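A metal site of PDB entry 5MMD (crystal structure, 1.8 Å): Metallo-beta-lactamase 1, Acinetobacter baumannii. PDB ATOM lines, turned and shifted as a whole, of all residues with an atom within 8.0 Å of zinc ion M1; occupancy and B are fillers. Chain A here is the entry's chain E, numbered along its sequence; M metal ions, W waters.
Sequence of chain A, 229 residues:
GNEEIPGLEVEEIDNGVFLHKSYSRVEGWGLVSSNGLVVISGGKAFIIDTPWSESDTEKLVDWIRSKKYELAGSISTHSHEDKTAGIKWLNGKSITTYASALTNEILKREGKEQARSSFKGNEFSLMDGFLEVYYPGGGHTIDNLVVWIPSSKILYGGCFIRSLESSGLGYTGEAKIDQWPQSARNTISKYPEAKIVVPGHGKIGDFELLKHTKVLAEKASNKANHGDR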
ATOM      1  N   VAL A  32     -12.704 -12.879 -13.363  1.00  0.00           N
ATOM      2  CA  VAL A  32     -12.399 -12.327 -14.670  1.00  0.00           C
ATOM      3  C   VAL A  32     -11.422 -13.278 -15.415  1.00  0.00           C
ATOM      4  O   VAL A  32     -10.572 -13.924 -14.800  1.00  0.00           O
ATOM      5  CB  VAL A  32     -11.751 -10.916 -14.518  1.00  0.00           C
ATOM      6  CG1 VAL A  32     -11.506 -10.270 -15.858  1.00  0.00           C
ATOM      7  CG2 VAL A  32     -12.587 -10.051 -13.624  1.00  0.00           C
ATOM      8  N   SER A  33     -11.558 -13.399 -16.728  1.00  0.00           N
ATOM      9  CA  SER A  33     -10.594 -14.171 -17.496  1.00  0.00           C
ATOM     10  C   SER A  33      -9.741 -13.223 -18.355  1.00  0.00           C
ATOM     11  O   SER A  33     -10.175 -12.135 -18.697  1.00  0.00           O
ATOM     12  CB  SER A  33     -11.284 -15.211 -18.384  1.00  0.00           C
ATOM     13  OG  SER A  33     -12.067 -14.587 -19.378  1.00  0.00           O
ATOM     14  N   SER A  34      -8.590 -13.697 -18.779  1.00  0.00           N
ATOM     15  CA  SER A  34      -7.696 -12.905 -19.624  1.00  0.00           C
ATOM     16  C   SER A  34      -7.158 -13.752 -20.742  1.00  0.00           C
ATOM     17  O   SER A  34      -6.828 -14.898 -20.499  1.00  0.00           O
ATOM     18  CB  SER A  34      -6.550 -12.357 -18.784  1.00  0.00           C
ATOM     19  OG  SER A  34      -5.458 -11.919 -19.587  1.00  0.00           O
ATOM     20  N   ASN A  35      -7.049 -13.182 -21.946  1.00  0.00           N
ATOM     21  CA  ASN A  35      -6.574 -13.897 -23.135  1.00  0.00           C
ATOM     22  C   ASN A  35      -5.115 -13.601 -23.457  1.00  0.00           C
ATOM     23  O   ASN A  35      -4.628 -12.512 -23.196  1.00  0.00           O
ATOM     24  CB  ASN A  35      -7.380 -13.517 -24.387  1.00  0.00           C
ATOM     25  CG  ASN A  35      -8.848 -13.828 -24.259  1.00  0.00           C
ATOM     26  OD1 ASN A  35      -9.249 -14.795 -23.622  1.00  0.00           O
ATOM     27  ND2 ASN A  35      -9.666 -12.996 -24.881  1.00  0.00           N
ATOM     28  N   ASP A  49       1.497 -12.248 -24.417  1.00  0.00           N
ATOM     29  CA  ASP A  49       0.988 -11.957 -23.053  1.00  0.00           C
ATOM     30  C   ASP A  49       1.042 -13.182 -22.169  1.00  0.00           C
ATOM     31  O   ASP A  49       0.673 -14.286 -22.584  1.00  0.00           O
ATOM     32  CB  ASP A  49      -0.419 -11.361 -23.104  1.00  0.00           C
ATOM     33  CG  ASP A  49      -0.374  -9.915 -23.488  1.00  0.00           C
ATOM     34  OD1 ASP A  49       0.738  -9.357 -23.387  1.00  0.00           O
ATOM     35  OD2 ASP A  49      -1.389  -9.335 -23.917  1.00  0.00           O
ATOM     36  N   TRP A  52      -2.308 -14.902 -16.177  1.00  0.00           N
ATOM     37  CA  TRP A  52      -2.497 -14.068 -15.005  1.00  0.00           C
ATOM     38  C   TRP A  52      -1.850 -14.587 -13.740  1.00  0.00           C
ATOM     39  O   TRP A  52      -2.130 -14.065 -12.672  1.00  0.00           O
ATOM     40  CB  TRP A  52      -3.994 -13.915 -14.723  1.00  0.00           C
ATOM     41  CG  TRP A  52      -4.453 -12.590 -14.226  1.00  0.00           C
ATOM     42  CD1 TRP A  52      -3.771 -11.714 -13.426  1.00  0.00           C
ATOM     43  CD2 TRP A  52      -5.726 -11.998 -14.481  1.00  0.00           C
ATOM     44  NE1 TRP A  52      -4.557 -10.612 -13.166  1.00  0.00           N
ATOM     45  CE2 TRP A  52      -5.755 -10.749 -13.818  1.00  0.00           C
ATOM     46  CE3 TRP A  52      -6.849 -12.412 -15.211  1.00  0.00           C
ATOM     47  CZ2 TRP A  52      -6.876  -9.901 -13.852  1.00  0.00           C
ATOM     48  CZ3 TRP A  52      -7.940 -11.569 -15.272  1.00  0.00           C
ATOM     49  CH2 TRP A  52      -7.949 -10.313 -14.595  1.00  0.00           C
ATOM     50  N   THR A  77       1.926  -6.920 -23.672  1.00  0.00           N
ATOM     51  CA  THR A  77       1.423  -5.827 -24.501  1.00  0.00           C
ATOM     52  C   THR A  77       0.988  -4.601 -23.702  1.00  0.00           C
ATOM     53  O   THR A  77       0.700  -3.558 -24.274  1.00  0.00           O
ATOM     54  CB  THR A  77       0.245  -6.321 -25.409  1.00  0.00           C
ATOM     55  OG1 THR A  77      -0.851  -6.767 -24.595  1.00  0.00           O
ATOM     56  CG2 THR A  77       0.709  -7.457 -26.270  1.00  0.00           C
ATOM     57  N   HIS A  78       0.917  -4.733 -22.370  1.00  0.00           N
ATOM     58  CA  HIS A  78       1.026  -3.530 -21.519  1.00  0.00           C
ATOM     59  C   HIS A  78       1.388  -3.999 -20.121  1.00  0.00           C
ATOM     60  O   HIS A  78       1.537  -5.211 -19.897  1.00  0.00           O
ATOM     61  CB  HIS A  78      -0.253  -2.672 -21.524  1.00  0.00           C
ATOM     62  CG  HIS A  78      -1.483  -3.329 -20.973  1.00  0.00           C
ATOM     63  ND1 HIS A  78      -2.166  -4.328 -21.632  1.00  0.00           N
ATOM     64  CD2 HIS A  78      -2.222  -3.045 -19.859  1.00  0.00           C
ATOM     65  CE1 HIS A  78      -3.227  -4.674 -20.924  1.00  0.00           C
ATOM     66  NE2 HIS A  78      -3.289  -3.893 -19.856  1.00  0.00           N
ATOM     67  N   HIS A  80      -0.161  -4.163 -17.109  1.00  0.00           N
ATOM     68  CA  HIS A  80      -1.089  -4.760 -16.125  1.00  0.00           C
ATOM     69  C   HIS A  80      -0.817  -6.242 -15.859  1.00  0.00           C
ATOM     70  O   HIS A  80      -0.333  -6.995 -16.725  1.00  0.00           O
ATOM     71  CB  HIS A  80      -2.543  -4.544 -16.527  1.00  0.00           C
ATOM     72  CG  HIS A  80      -2.992  -3.122 -16.393  1.00  0.00           C
ATOM     73  ND1 HIS A  80      -4.090  -2.619 -17.048  1.00  0.00           N
ATOM     74  CD2 HIS A  80      -2.488  -2.103 -15.642  1.00  0.00           C
ATOM     75  CE1 HIS A  80      -4.258  -1.348 -16.713  1.00  0.00           C
ATOM     76  NE2 HIS A  80      -3.286  -1.009 -15.872  1.00  0.00           N
ATOM     77  N   GLU A  81      -1.071  -6.619 -14.622  1.00  0.00           N
ATOM     78  CA  GLU A  81      -0.778  -7.948 -14.111  1.00  0.00           C
ATOM     79  C   GLU A  81      -1.394  -9.083 -14.942  1.00  0.00           C
ATOM     80  O   GLU A  81      -0.829 -10.176 -14.985  1.00  0.00           O
ATOM     81  CB  GLU A  81      -1.259  -8.051 -12.680  1.00  0.00           C
ATOM     82  CG  GLU A  81      -0.799  -9.268 -11.915  1.00  0.00           C
ATOM     83  CD  GLU A  81       0.675  -9.281 -11.579  1.00  0.00           C
ATOM     84  OE1 GLU A  81       1.093 -10.293 -11.000  1.00  0.00           O
ATOM     85  OE2 GLU A  81       1.411  -8.300 -11.830  1.00  0.00           O
ATOM     86  N   ASP A  82      -2.517  -8.828 -15.606  1.00  0.00           N
ATOM     87  CA  ASP A  82      -3.145  -9.896 -16.392  1.00  0.00           C
ATOM     88  C   ASP A  82      -2.267 -10.298 -17.598  1.00  0.00           C
ATOM     89  O   ASP A  82      -2.460 -11.369 -18.126  1.00  0.00           O
ATOM     90  CB  ASP A  82      -4.601  -9.555 -16.843  1.00  0.00           C
ATOM     91  CG  ASP A  82      -4.740  -8.243 -17.588  1.00  0.00           C
ATOM     92  OD1 ASP A  82      -3.982  -7.303 -17.259  1.00  0.00           O
ATOM     93  OD2 ASP A  82      -5.697  -8.120 -18.434  1.00  0.00           O
ATOM     94  N   LYS A  83      -1.308  -9.480 -18.000  1.00  0.00           N
ATOM     95  CA  LYS A  83      -0.473  -9.770 -19.190  1.00  0.00           C
ATOM     96  C   LYS A  83       1.019  -9.923 -18.874  1.00  0.00           C
ATOM     97  O   LYS A  83       1.816 -10.350 -19.751  1.00  0.00           O
ATOM     98  CB  LYS A  83      -0.654  -8.650 -20.219  1.00  0.00           C
ATOM     99  CG  LYS A  83      -2.068  -8.334 -20.621  1.00  0.00           C
ATOM    100  CD  LYS A  83      -2.892  -9.557 -21.068  1.00  0.00           C
ATOM    101  CE  LYS A  83      -4.302  -9.119 -21.491  1.00  0.00           C
ATOM    102  NZ  LYS A  83      -5.162 -10.274 -21.697  1.00  0.00           N
ATOM    103  N   HIS A 140      -6.795   1.861 -23.642  1.00  0.00           N
ATOM    104  CA  HIS A 140      -6.891   1.159 -22.371  1.00  0.00           C
ATOM    105  C   HIS A 140      -5.851   1.687 -21.378  1.00  0.00           C
ATOM    106  O   HIS A 140      -6.160   1.860 -20.198  1.00  0.00           O
ATOM    107  CB  HIS A 140      -6.716  -0.309 -22.615  1.00  0.00           C
ATOM    108  CG  HIS A 140      -6.601  -1.127 -21.372  1.00  0.00           C
ATOM    109  ND1 HIS A 140      -7.662  -1.334 -20.515  1.00  0.00           N
ATOM    110  CD2 HIS A 140      -5.540  -1.778 -20.834  1.00  0.00           C
ATOM    111  CE1 HIS A 140      -7.243  -2.087 -19.499  1.00  0.00           C
ATOM    112  NE2 HIS A 140      -5.962  -2.372 -19.667  1.00  0.00           N
ATOM    113  N   THR A 141      -4.611   1.858 -21.882  1.00  0.00           N
ATOM    114  CA  THR A 141      -3.504   2.419 -21.125  1.00  0.00           C
ATOM    115  C   THR A 141      -2.614   3.211 -22.074  1.00  0.00           C
ATOM    116  O   THR A 141      -2.720   3.121 -23.314  1.00  0.00           O
ATOM    117  CB  THR A 141      -2.654   1.332 -20.397  1.00  0.00           C
ATOM    118  OG1 THR A 141      -2.149   0.366 -21.347  1.00  0.00           O
ATOM    119  CG2 THR A 141      -3.478   0.637 -19.308  1.00  0.00           C
ATOM    120  N   TYR A 156      -3.862  -9.536 -32.605  1.00  0.00           N
ATOM    121  CA  TYR A 156      -4.049  -9.578 -31.165  1.00  0.00           C
ATOM    122  C   TYR A 156      -4.154  -8.142 -30.650  1.00  0.00           C
ATOM    123  O   TYR A 156      -3.172  -7.402 -30.650  1.00  0.00           O
ATOM    124  CB  TYR A 156      -2.927 -10.312 -30.454  1.00  0.00           C
ATOM    125  CG  TYR A 156      -3.116 -10.266 -28.950  1.00  0.00           C
ATOM    126  CD1 TYR A 156      -4.073 -11.066 -28.308  1.00  0.00           C
ATOM    127  CD2 TYR A 156      -2.384  -9.374 -28.163  1.00  0.00           C
ATOM    128  CE1 TYR A 156      -4.256 -11.019 -26.931  1.00  0.00           C
ATOM    129  CE2 TYR A 156      -2.575  -9.298 -26.796  1.00  0.00           C
ATOM    130  CZ  TYR A 156      -3.493 -10.131 -26.171  1.00  0.00           C
ATOM    131  OH  TYR A 156      -3.654 -10.033 -24.812  1.00  0.00           O
ATOM    132  N   GLY A 158      -5.174  -7.167 -27.573  1.00  0.00           N
ATOM    133  CA  GLY A 158      -5.026  -6.975 -26.155  1.00  0.00           C
ATOM    134  C   GLY A 158      -6.143  -6.099 -25.594  1.00  0.00           C
ATOM    135  O   GLY A 158      -7.209  -5.954 -26.192  1.00  0.00           O
ATOM    136  N   CYS A 159      -5.902  -5.526 -24.432  1.00  0.00           N
ATOM    137  CA  CYS A 159      -7.014  -4.878 -23.748  1.00  0.00           C
ATOM    138  C   CYS A 159      -7.332  -3.542 -24.360  1.00  0.00           C
ATOM    139  O   CYS A 159      -8.290  -2.913 -23.968  1.00  0.00           O
ATOM    140  CB  CYS A 159      -6.702  -4.765 -22.277  1.00  0.00           C
ATOM    141  SG  CYS A 159      -6.288  -6.376 -21.649  1.00  0.00           S
ATOM    142  N   PHE A 160      -6.544  -3.152 -25.364  1.00  0.00           N
ATOM    143  CA  PHE A 160      -6.837  -2.004 -26.208  1.00  0.00           C
ATOM    144  C   PHE A 160      -8.098  -2.222 -27.032  1.00  0.00           C
ATOM    145  O   PHE A 160      -8.710  -1.261 -27.531  1.00  0.00           O
ATOM    146  CB  PHE A 160      -5.649  -1.753 -27.162  1.00  0.00           C
ATOM    147  CG  PHE A 160      -5.878  -0.643 -28.155  1.00  0.00           C
ATOM    148  CD1 PHE A 160      -5.884   0.674 -27.741  1.00  0.00           C
ATOM    149  CD2 PHE A 160      -6.058  -0.918 -29.518  1.00  0.00           C
ATOM    150  CE1 PHE A 160      -6.086   1.706 -28.639  1.00  0.00           C
ATOM    151  CE2 PHE A 160      -6.251   0.115 -30.421  1.00  0.00           C
ATOM    152  CZ  PHE A 160      -6.272   1.437 -29.972  1.00  0.00           C
ATOM    153  N   ARG A 162     -11.853  -4.120 -27.278  1.00  0.00           N
ATOM    154  CA  ARG A 162     -12.947  -4.710 -26.533  1.00  0.00           C
ATOM    155  C   ARG A 162     -13.709  -5.758 -27.328  1.00  0.00           C
ATOM    156  O   ARG A 162     -13.851  -5.652 -28.550  1.00  0.00           O
ATOM    157  CB  ARG A 162     -13.918  -3.623 -26.097  1.00  0.00           C
ATOM    158  CG  ARG A 162     -13.240  -2.562 -25.208  1.00  0.00           C
ATOM    159  CD  ARG A 162     -12.817  -3.141 -23.855  1.00  0.00           C
ATOM    160  NE  ARG A 162     -14.001  -3.425 -23.036  1.00  0.00           N
ATOM    161  CZ  ARG A 162     -14.016  -4.150 -21.923  1.00  0.00           C
ATOM    162  NH1 ARG A 162     -12.893  -4.705 -21.426  1.00  0.00           N
ATOM    163  NH2 ARG A 162     -15.164  -4.294 -21.282  1.00  0.00           N
ATOM    164  N   TYR A 171     -12.128  -1.596 -17.531  1.00  0.00           N
ATOM    165  CA  TYR A 171     -11.387  -0.848 -16.510  1.00  0.00           C
ATOM    166  C   TYR A 171     -10.706   0.376 -17.101  1.00  0.00           C
ATOM    167  O   TYR A 171      -9.779   0.258 -17.905  1.00  0.00           O
ATOM    168  CB  TYR A 171     -10.339  -1.728 -15.839  1.00  0.00           C
ATOM    169  CG  TYR A 171      -9.427  -0.928 -14.917  1.00  0.00           C
ATOM    170  CD1 TYR A 171      -9.930  -0.294 -13.783  1.00  0.00           C
ATOM    171  CD2 TYR A 171      -8.065  -0.771 -15.198  1.00  0.00           C
ATOM    172  CE1 TYR A 171      -9.091   0.432 -12.929  1.00  0.00           C
ATOM    173  CE2 TYR A 171      -7.220  -0.037 -14.355  1.00  0.00           C
ATOM    174  CZ  TYR A 171      -7.746   0.570 -13.242  1.00  0.00           C
ATOM    175  OH  TYR A 171      -6.931   1.296 -12.391  1.00  0.00           O
ATOM    176  N   PRO A 199      -9.504  -9.948 -28.501  1.00  0.00           N
ATOM    177  CA  PRO A 199      -9.504  -8.915 -27.480  1.00  0.00           C
ATOM    178  C   PRO A 199      -8.727  -9.392 -26.266  1.00  0.00           C
ATOM    179  O   PRO A 199      -8.495 -10.593 -26.174  1.00  0.00           O
ATOM    180  CB  PRO A 199     -10.999  -8.757 -27.175  1.00  0.00           C
ATOM    181  CG  PRO A 199     -11.526 -10.154 -27.298  1.00  0.00           C
ATOM    182  CD  PRO A 199     -10.745 -10.743 -28.490  1.00  0.00           C
ATOM    183  N   GLY A 200      -8.331  -8.500 -25.359  1.00  0.00           N
ATOM    184  CA  GLY A 200      -7.615  -8.886 -24.161  1.00  0.00           C
ATOM    185  C   GLY A 200      -8.461  -9.699 -23.198  1.00  0.00           C
ATOM    186  O   GLY A 200      -7.948 -10.532 -22.442  1.00  0.00           O
ATOM    187  N   HIS A 201      -9.769  -9.447 -23.272  1.00  0.00           N
ATOM    188  CA  HIS A 201     -10.813 -10.043 -22.424  1.00  0.00           C
ATOM    189  C   HIS A 201     -12.016 -10.349 -23.298  1.00  0.00           C
ATOM    190  O   HIS A 201     -12.501  -9.481 -24.060  1.00  0.00           O
ATOM    191  CB  HIS A 201     -11.193  -9.089 -21.286  1.00  0.00           C
ATOM    192  CG  HIS A 201     -10.058  -8.744 -20.386  1.00  0.00           C
ATOM    193  ND1 HIS A 201      -9.553  -9.638 -19.456  1.00  0.00           N
ATOM    194  CD2 HIS A 201      -9.270  -7.637 -20.305  1.00  0.00           C
ATOM    195  CE1 HIS A 201      -8.548  -9.079 -18.811  1.00  0.00           C
ATOM    196  NE2 HIS A 201      -8.365  -7.856 -19.301  1.00  0.00           N
HETATM  197 ZN    ZN M   1      -6.598  -6.570 -19.318  1.00  0.00          ZN
HETATM  198 ZN    ZN M   2      -4.978  -3.603 -18.574  1.00  0.00          ZN
HETATM  199  O   HOH W   1      -5.912  -5.066 -18.077  1.00  0.00           O
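The backbone carbonyl oxygen of Asp 82 is in hydrogen-bond range of the side-chain hydroxyl of Ser 34. ND1 of His 201 is in hydrogen-bond range of O of Ser 33 (2.7 Å). OD2 of Asp 82 lies close to NZ of Lys 83 (3.9 Å).
Zinc ion M1 is bound by OD2 of Asp 82 (2.0 Å), water W1 (2.1 Å), NE2 of His 201 (2.2 Å) and SG of Cys 159 (2.4 Å).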
